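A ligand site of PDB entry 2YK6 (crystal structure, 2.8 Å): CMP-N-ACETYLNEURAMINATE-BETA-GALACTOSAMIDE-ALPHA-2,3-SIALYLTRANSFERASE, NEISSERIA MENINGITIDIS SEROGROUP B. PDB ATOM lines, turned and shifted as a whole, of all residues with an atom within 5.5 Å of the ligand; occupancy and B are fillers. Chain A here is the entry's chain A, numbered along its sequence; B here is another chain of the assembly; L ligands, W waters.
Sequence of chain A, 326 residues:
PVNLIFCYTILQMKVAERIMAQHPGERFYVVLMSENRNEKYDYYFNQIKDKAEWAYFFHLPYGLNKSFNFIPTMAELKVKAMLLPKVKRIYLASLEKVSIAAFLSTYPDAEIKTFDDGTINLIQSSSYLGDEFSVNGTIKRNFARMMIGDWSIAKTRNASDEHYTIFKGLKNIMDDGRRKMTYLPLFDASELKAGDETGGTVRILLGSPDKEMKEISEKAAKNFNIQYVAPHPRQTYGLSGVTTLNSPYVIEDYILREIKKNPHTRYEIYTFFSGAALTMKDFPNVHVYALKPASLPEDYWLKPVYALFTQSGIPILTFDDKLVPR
The side-chain carboxylate (OE1) of Glu 252 is in hydrogen-bond range of an oxygen (O10) of the ligand, at 2.4 Å.
An oxygen (O11) of the ligand lies within hydrogen-bond range of the backbone NH (N) of Ile 251.
NE of Arg 234 lies within salt-bridge range of O3 of the ligand.
The backbone NH (N) of Gly 275 sits at hydrogen-bond distance from an oxygen (O6) of the ligand, at 2.9 Å.
The backbone carbonyl oxygen (O) of Ala 230 is in hydrogen-bond range of a nitrogen (N3) of the ligand.
The side-chain amide nitrogen (ND2) of Asn 69 of chain B is in hydrogen-bond range of an oxygen (O1) of the ligand, at 3.0 Å.
A ring nitrogen (NE2) of His 232 lies close to an oxygen (O2) of the ligand.
An oxygen (O5) of the ligand sits at hydrogen-bond distance from the side-chain hydroxyl (OG) of Ser 274 (3.1 Å).
Water W1 lies within hydrogen-bond range of O3 of the ligand (2.5 Å), OD1 of Asn 69 of chain B (2.8 Å) and NE of Arg 234 (3.2 Å).
OE2 of Glu 252 is in hydrogen-bond range of OG1 of Thr 279 (2.8 Å).
O of Ala 230 sits at hydrogen-bond distance from N of Gly 207.
N of Thr 119 is in hydrogen-bond range of O of Asn 69 of chain B (3.5 Å).
The side-chain amide nitrogen (NE2) of Gln 235 lies close to the backbone NH (N) of His 232 (2.7 Å).
The side-chain hydroxyl of Ser 274 sits close to the backbone NH of Ala 276, 3.3 Å away.
The side-chain hydroxyl of Thr 279 lies within hydrogen-bond range of the backbone carbonyl oxygen of Ala 276 (3.0 Å).
The backbone NH (N) of Gly 207 lies close to a nitrogen (N3) of the ligand.
Leu 206 touches the ligand.
Pro 231 touches the ligand (C to N3, 3.6 Å).
Pro 233 touches the ligand (CD to C6, 3.7 Å).
Val 250 touches the ligand (CB to O11, 3.4 Å).
CB of Ala 276 touches C3 of the ligand (3.7 Å).
Thr 279 touches the ligand.
Leu 11 of chain B touches the ligand.
Phe 70 of chain B touches the ligand.
Within 4 Å of the ligand: Leu 206, Gly 207, Ala 230, Pro 231, His 232, Pro 233, Arg 234, Val 250, Ile 251, Glu 252, Ser 274, Gly 275, Ala 276, Thr 279, Leu 11 of chain B, Asn 69 of chain B and Phe 70 of chain B.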
ATOM      1  N   THR A 119       7.566  24.161  32.859  1.00  0.00           N
ATOM      2  CA  THR A 119       7.982  23.274  33.939  1.00  0.00           C
ATOM      3  C   THR A 119       9.330  23.664  34.562  1.00  0.00           C
ATOM      4  O   THR A 119       9.573  23.364  35.724  1.00  0.00           O
ATOM      5  CB  THR A 119       8.104  21.849  33.454  1.00  0.00           C
ATOM      6  OG1 THR A 119       8.943  21.823  32.311  1.00  0.00           O
ATOM      7  CG2 THR A 119       6.780  21.327  33.056  1.00  0.00           C
ATOM      8  N   LEU A 206       1.946  10.385  24.278  1.00  0.00           N
ATOM      9  CA  LEU A 206       2.453  11.700  23.916  1.00  0.00           C
ATOM     10  C   LEU A 206       3.786  11.507  23.213  1.00  0.00           C
ATOM     11  O   LEU A 206       4.670  10.793  23.699  1.00  0.00           O
ATOM     12  CB  LEU A 206       2.627  12.576  25.134  1.00  0.00           C
ATOM     13  CG  LEU A 206       1.343  12.744  25.948  1.00  0.00           C
ATOM     14  CD1 LEU A 206       1.554  13.781  27.064  1.00  0.00           C
ATOM     15  CD2 LEU A 206       0.148  13.129  25.057  1.00  0.00           C
ATOM     16  N   GLY A 207       3.900  12.105  22.031  1.00  0.00           N
ATOM     17  CA  GLY A 207       5.134  12.025  21.259  1.00  0.00           C
ATOM     18  C   GLY A 207       6.268  12.800  21.920  1.00  0.00           C
ATOM     19  O   GLY A 207       6.025  13.795  22.607  1.00  0.00           O
ATOM     20  N   PRO A 209       9.788  15.048  21.322  1.00  0.00           N
ATOM     21  CA  PRO A 209      10.461  15.790  20.269  1.00  0.00           C
ATOM     22  C   PRO A 209      11.811  15.182  19.872  1.00  0.00           C
ATOM     23  O   PRO A 209      12.256  15.422  18.773  1.00  0.00           O
ATOM     24  CB  PRO A 209      10.655  17.187  20.867  1.00  0.00           C
ATOM     25  CG  PRO A 209       9.951  17.195  22.182  1.00  0.00           C
ATOM     26  CD  PRO A 209       9.768  15.773  22.597  1.00  0.00           C
ATOM     27  N   ALA A 230      -0.195  11.336  20.165  1.00  0.00           N
ATOM     28  CA  ALA A 230      -0.343  12.800  20.075  1.00  0.00           C
ATOM     29  C   ALA A 230       1.044  13.378  19.886  1.00  0.00           C
ATOM     30  O   ALA A 230       1.860  13.302  20.801  1.00  0.00           O
ATOM     31  CB  ALA A 230      -1.009  13.424  21.329  1.00  0.00           C
ATOM     32  N   PRO A 231       1.322  13.923  18.702  1.00  0.00           N
ATOM     33  CA  PRO A 231       2.690  14.373  18.470  1.00  0.00           C
ATOM     34  C   PRO A 231       3.049  15.675  19.215  1.00  0.00           C
ATOM     35  O   PRO A 231       2.176  16.532  19.426  1.00  0.00           O
ATOM     36  CB  PRO A 231       2.768  14.507  16.957  1.00  0.00           C
ATOM     37  CG  PRO A 231       1.380  14.576  16.485  1.00  0.00           C
ATOM     38  CD  PRO A 231       0.441  14.224  17.564  1.00  0.00           C
ATOM     39  N   HIS A 232       4.300  15.803  19.656  1.00  0.00           N
ATOM     40  CA  HIS A 232       4.748  17.029  20.325  1.00  0.00           C
ATOM     41  C   HIS A 232       4.742  18.227  19.357  1.00  0.00           C
ATOM     42  O   HIS A 232       4.991  18.041  18.162  1.00  0.00           O
ATOM     43  CB  HIS A 232       6.131  16.844  20.951  1.00  0.00           C
ATOM     44  CG  HIS A 232       6.480  17.902  21.949  1.00  0.00           C
ATOM     45  ND1 HIS A 232       6.397  17.702  23.313  1.00  0.00           N
ATOM     46  CD2 HIS A 232       6.891  19.188  21.779  1.00  0.00           C
ATOM     47  CE1 HIS A 232       6.743  18.807  23.942  1.00  0.00           C
ATOM     48  NE2 HIS A 232       7.051  19.717  23.031  1.00  0.00           N
ATOM     49  N   PRO A 233       4.423  19.451  19.848  1.00  0.00           N
ATOM     50  CA  PRO A 233       4.476  20.568  18.877  1.00  0.00           C
ATOM     51  C   PRO A 233       5.894  20.841  18.379  1.00  0.00           C
ATOM     52  O   PRO A 233       6.056  21.305  17.251  1.00  0.00           O
ATOM     53  CB  PRO A 233       3.913  21.780  19.658  1.00  0.00           C
ATOM     54  CG  PRO A 233       3.139  21.178  20.784  1.00  0.00           C
ATOM     55  CD  PRO A 233       3.832  19.877  21.141  1.00  0.00           C
ATOM     56  N   ARG A 234       6.897  20.524  19.201  1.00  0.00           N
ATOM     57  CA  ARG A 234       8.301  20.662  18.763  1.00  0.00           C
ATOM     58  C   ARG A 234       8.748  19.448  17.945  1.00  0.00           C
ATOM     59  O   ARG A 234       9.860  19.430  17.451  1.00  0.00           O
ATOM     60  CB  ARG A 234       9.247  20.905  19.942  1.00  0.00           C
ATOM     61  CG  ARG A 234       9.008  22.265  20.617  1.00  0.00           C
ATOM     62  CD  ARG A 234      10.070  22.656  21.638  1.00  0.00           C
ATOM     63  NE  ARG A 234       9.956  21.908  22.889  1.00  0.00           N
ATOM     64  CZ  ARG A 234      10.745  20.886  23.217  1.00  0.00           C
ATOM     65  NH1 ARG A 234      11.715  20.527  22.380  1.00  0.00           N
ATOM     66  NH2 ARG A 234      10.586  20.237  24.366  1.00  0.00           N
ATOM     67  N   GLN A 235       7.858  18.448  17.803  1.00  0.00           N
ATOM     68  CA  GLN A 235       8.140  17.151  17.168  1.00  0.00           C
ATOM     69  C   GLN A 235       8.023  17.238  15.681  1.00  0.00           C
ATOM     70  O   GLN A 235       7.164  17.942  15.164  1.00  0.00           O
ATOM     71  CB  GLN A 235       7.203  16.059  17.685  1.00  0.00           C
ATOM     72  CG  GLN A 235       7.288  14.733  16.946  1.00  0.00           C
ATOM     73  CD  GLN A 235       6.584  13.612  17.672  1.00  0.00           C
ATOM     74  OE1 GLN A 235       6.576  12.483  17.213  1.00  0.00           O
ATOM     75  NE2 GLN A 235       5.988  13.925  18.795  1.00  0.00           N
ATOM     76  N   TYR A 249      -4.951  21.553  18.012  1.00  0.00           N
ATOM     77  CA  TYR A 249      -4.849  21.714  19.475  1.00  0.00           C
ATOM     78  C   TYR A 249      -3.611  21.079  20.126  1.00  0.00           C
ATOM     79  O   TYR A 249      -3.041  20.065  19.635  1.00  0.00           O
ATOM     80  CB  TYR A 249      -6.089  21.205  20.216  1.00  0.00           C
ATOM     81  CG  TYR A 249      -7.375  21.683  19.615  1.00  0.00           C
ATOM     82  CD1 TYR A 249      -7.722  23.029  19.644  1.00  0.00           C
ATOM     83  CD2 TYR A 249      -8.229  20.785  18.987  1.00  0.00           C
ATOM     84  CE1 TYR A 249      -8.895  23.460  19.073  1.00  0.00           C
ATOM     85  CE2 TYR A 249      -9.387  21.202  18.425  1.00  0.00           C
ATOM     86  CZ  TYR A 249      -9.737  22.535  18.459  1.00  0.00           C
ATOM     87  OH  TYR A 249     -10.935  22.939  17.886  1.00  0.00           O
ATOM     88  N   VAL A 250      -3.186  21.683  21.218  1.00  0.00           N
ATOM     89  CA  VAL A 250      -2.252  21.009  22.081  1.00  0.00           C
ATOM     90  C   VAL A 250      -3.034  19.924  22.822  1.00  0.00           C
ATOM     91  O   VAL A 250      -4.301  19.951  22.822  1.00  0.00           O
ATOM     92  CB  VAL A 250      -1.484  21.958  23.032  1.00  0.00           C
ATOM     93  CG1 VAL A 250      -0.440  22.733  22.230  1.00  0.00           C
ATOM     94  CG2 VAL A 250      -2.424  22.861  23.833  1.00  0.00           C
ATOM     95  N   ILE A 251      -2.307  18.978  23.430  1.00  0.00           N
ATOM     96  CA  ILE A 251      -2.964  17.834  23.981  1.00  0.00           C
ATOM     97  C   ILE A 251      -4.057  18.169  24.975  1.00  0.00           C
ATOM     98  O   ILE A 251      -5.156  17.663  24.834  1.00  0.00           O
ATOM     99  CB  ILE A 251      -2.021  16.748  24.509  1.00  0.00           C
ATOM    100  CG1 ILE A 251      -2.865  15.533  24.894  1.00  0.00           C
ATOM    101  CG2 ILE A 251      -1.163  17.219  25.715  1.00  0.00           C
ATOM    102  CD1 ILE A 251      -3.654  14.951  23.712  1.00  0.00           C
ATOM    103  N   GLU A 252      -3.776  19.033  25.939  1.00  0.00           N
ATOM    104  CA  GLU A 252      -4.771  19.347  26.962  1.00  0.00           C
ATOM    105  C   GLU A 252      -6.076  19.825  26.312  1.00  0.00           C
ATOM    106  O   GLU A 252      -7.168  19.348  26.675  1.00  0.00           O
ATOM    107  CB  GLU A 252      -4.286  20.406  27.965  1.00  0.00           C
ATOM    108  CG  GLU A 252      -3.040  20.094  28.695  1.00  0.00           C
ATOM    109  CD  GLU A 252      -1.804  20.613  27.976  1.00  0.00           C
ATOM    110  OE1 GLU A 252      -1.848  20.774  26.729  1.00  0.00           O
ATOM    111  OE2 GLU A 252      -0.775  20.835  28.651  1.00  0.00           O
ATOM    112  N   PHE A 273       7.515  11.609  30.604  1.00  0.00           N
ATOM    113  CA  PHE A 273       7.788  12.735  31.467  1.00  0.00           C
ATOM    114  C   PHE A 273       7.600  14.087  30.765  1.00  0.00           C
ATOM    115  O   PHE A 273       8.393  15.018  30.963  1.00  0.00           O
ATOM    116  CB  PHE A 273       9.197  12.612  32.106  1.00  0.00           C
ATOM    117  CG  PHE A 273       9.331  11.433  33.043  1.00  0.00           C
ATOM    118  CD1 PHE A 273       8.908  11.505  34.356  1.00  0.00           C
ATOM    119  CD2 PHE A 273       9.863  10.234  32.594  1.00  0.00           C
ATOM    120  CE1 PHE A 273       9.044  10.395  35.236  1.00  0.00           C
ATOM    121  CE2 PHE A 273       9.998   9.100  33.470  1.00  0.00           C
ATOM    122  CZ  PHE A 273       9.592   9.206  34.799  1.00  0.00           C
ATOM    123  N   SER A 274       6.558  14.216  29.940  1.00  0.00           N
ATOM    124  CA  SER A 274       6.203  15.542  29.428  1.00  0.00           C
ATOM    125  C   SER A 274       5.445  16.397  30.424  1.00  0.00           C
ATOM    126  O   SER A 274       4.531  15.896  31.101  1.00  0.00           O
ATOM    127  CB  SER A 274       5.368  15.434  28.155  1.00  0.00           C
ATOM    128  OG  SER A 274       4.867  16.722  27.793  1.00  0.00           O
ATOM    129  N   GLY A 275       5.780  17.689  30.449  1.00  0.00           N
ATOM    130  CA  GLY A 275       5.054  18.663  31.255  1.00  0.00           C
ATOM    131  C   GLY A 275       3.527  18.532  31.266  1.00  0.00           C
ATOM    132  O   GLY A 275       2.850  18.921  32.231  1.00  0.00           O
ATOM    133  N   ALA A 276       2.995  17.958  30.180  1.00  0.00           N
ATOM    134  CA  ALA A 276       1.570  17.813  29.987  1.00  0.00           C
ATOM    135  C   ALA A 276       0.940  16.970  31.097  1.00  0.00           C
ATOM    136  O   ALA A 276      -0.211  17.160  31.463  1.00  0.00           O
ATOM    137  CB  ALA A 276       1.294  17.199  28.644  1.00  0.00           C
ATOM    138  N   THR A 279      -0.020  19.340  33.780  1.00  0.00           N
ATOM    139  CA  THR A 279      -1.180  20.211  33.605  1.00  0.00           C
ATOM    140  C   THR A 279      -2.476  19.424  33.541  1.00  0.00           C
ATOM    141  O   THR A 279      -3.563  19.973  33.696  1.00  0.00           O
ATOM    142  CB  THR A 279      -1.040  20.987  32.356  1.00  0.00           C
ATOM    143  OG1 THR A 279      -0.555  20.107  31.347  1.00  0.00           O
ATOM    144  CG2 THR A 279      -0.034  22.094  32.571  1.00  0.00           C
ATOM    145  N   LEU B  11       1.876  27.477  25.402  1.00  0.00           N
ATOM    146  CA  LEU B  11       1.190  27.635  26.696  1.00  0.00           C
ATOM    147  C   LEU B  11       1.243  29.063  27.247  1.00  0.00           C
ATOM    148  O   LEU B  11       0.246  29.562  27.823  1.00  0.00           O
ATOM    149  CB  LEU B  11       1.621  26.615  27.742  1.00  0.00           C
ATOM    150  CG  LEU B  11       1.135  25.167  27.527  1.00  0.00           C
ATOM    151  CD1 LEU B  11       1.210  24.360  28.811  1.00  0.00           C
ATOM    152  CD2 LEU B  11      -0.266  25.170  27.036  1.00  0.00           C
ATOM    153  N   LYS B  40       0.020  23.814  14.858  1.00  0.00           N
ATOM    154  CA  LYS B  40      -0.194  24.028  16.292  1.00  0.00           C
ATOM    155  C   LYS B  40       0.129  25.442  16.755  1.00  0.00           C
ATOM    156  O   LYS B  40      -0.689  26.086  17.409  1.00  0.00           O
ATOM    157  CB  LYS B  40       0.603  23.013  17.107  1.00  0.00           C
ATOM    158  CG  LYS B  40      -0.174  21.754  17.372  1.00  0.00           C
ATOM    159  CD  LYS B  40       0.727  20.564  17.619  1.00  0.00           C
ATOM    160  CE  LYS B  40      -0.055  19.254  17.442  1.00  0.00           C
ATOM    161  NZ  LYS B  40      -1.430  19.339  18.084  1.00  0.00           N
ATOM    162  N   ASN B  69      12.436  26.511  28.346  1.00  0.00           N
ATOM    163  CA  ASN B  69      11.212  26.714  29.121  1.00  0.00           C
ATOM    164  C   ASN B  69      10.760  25.442  29.811  1.00  0.00           C
ATOM    165  O   ASN B  69       9.917  25.492  30.685  1.00  0.00           O
ATOM    166  CB  ASN B  69      10.080  27.197  28.251  1.00  0.00           C
ATOM    167  CG  ASN B  69       9.569  26.113  27.348  1.00  0.00           C
ATOM    168  OD1 ASN B  69      10.072  25.955  26.243  1.00  0.00           O
ATOM    169  ND2 ASN B  69       8.590  25.346  27.829  1.00  0.00           N
ATOM    170  N   PHE B  70      11.274  24.302  29.387  1.00  0.00           N
ATOM    171  CA  PHE B  70      10.896  23.036  29.971  1.00  0.00           C
ATOM    172  C   PHE B  70      12.099  22.534  30.688  1.00  0.00           C
ATOM    173  O   PHE B  70      13.162  23.129  30.589  1.00  0.00           O
ATOM    174  CB  PHE B  70      10.484  22.032  28.905  1.00  0.00           C
ATOM    175  CG  PHE B  70      11.395  22.013  27.714  1.00  0.00           C
ATOM    176  CD1 PHE B  70      12.539  21.221  27.712  1.00  0.00           C
ATOM    177  CD2 PHE B  70      11.103  22.788  26.599  1.00  0.00           C
ATOM    178  CE1 PHE B  70      13.372  21.193  26.618  1.00  0.00           C
ATOM    179  CE2 PHE B  70      11.916  22.783  25.496  1.00  0.00           C
ATOM    180  CZ  PHE B  70      13.065  21.982  25.493  1.00  0.00           C
ATOM    181  N   ILE B  71      11.961  21.429  31.419  1.00  0.00           N
ATOM    182  CA  ILE B  71      13.123  20.841  32.056  1.00  0.00           C
ATOM    183  C   ILE B  71      13.822  19.914  31.007  1.00  0.00           C
ATOM    184  O   ILE B  71      13.217  18.972  30.495  1.00  0.00           O
ATOM    185  CB  ILE B  71      12.720  20.119  33.378  1.00  0.00           C
ATOM    186  CG1 ILE B  71      12.023  21.080  34.358  1.00  0.00           C
ATOM    187  CG2 ILE B  71      13.925  19.522  34.032  1.00  0.00           C
ATOM    188  CD1 ILE B  71      11.316  20.367  35.509  1.00  0.00           C
HETATM  189  O1  LIG L   1       7.312  22.690  27.536  1.00  0.00           O
HETATM  190  P1  LIG L   1       7.563  21.776  26.200  1.00  0.00           P
HETATM  191  O2  LIG L   1       6.153  21.467  25.638  1.00  0.00           O
HETATM  192  O3  LIG L   1       8.283  22.499  25.120  1.00  0.00           O
HETATM  193  O4  LIG L   1       8.220  20.363  26.666  1.00  0.00           O
HETATM  194  P2  LIG L   1       7.291  19.415  27.570  1.00  0.00           P
HETATM  195  O5  LIG L   1       7.672  17.911  27.023  1.00  0.00           O
HETATM  196  O6  LIG L   1       7.487  19.622  29.056  1.00  0.00           O
HETATM  197  O7  LIG L   1       5.707  19.784  27.028  1.00  0.00           O
HETATM  198  C1  LIG L   1       4.762  20.865  27.593  1.00  0.00           C
HETATM  199  C2  LIG L   1       3.456  21.196  26.748  1.00  0.00           C
HETATM  200  O8  LIG L   1       3.491  20.666  25.428  1.00  0.00           O
HETATM  201  C3  LIG L   1       2.245  20.513  27.357  1.00  0.00           C
HETATM  202  O9  LIG L   1       1.679  21.321  28.381  1.00  0.00           O
HETATM  203  C4  LIG L   1       1.276  20.291  26.183  1.00  0.00           C
HETATM  204  O10 LIG L   1       0.354  21.338  25.898  1.00  0.00           O
HETATM  205  C5  LIG L   1       2.178  20.314  25.017  1.00  0.00           C
HETATM  206  N1  LIG L   1       2.310  18.964  24.470  1.00  0.00           N
HETATM  207  C6  LIG L   1       1.406  18.518  23.541  1.00  0.00           C
HETATM  208  O11 LIG L   1       0.457  19.232  23.201  1.00  0.00           O
HETATM  209  N2  LIG L   1       1.585  17.243  22.994  1.00  0.00           N
HETATM  210  C7  LIG L   1       2.636  16.440  23.349  1.00  0.00           C
HETATM  211  N3  LIG L   1       2.792  15.256  22.807  1.00  0.00           N
HETATM  212  C8  LIG L   1       3.540  16.885  24.278  1.00  0.00           C
HETATM  213  C9  LIG L   1       3.382  18.150  24.829  1.00  0.00           C
HETATM  214  O   HOH W   1       8.918  24.691  24.011  1.00  0.00           O
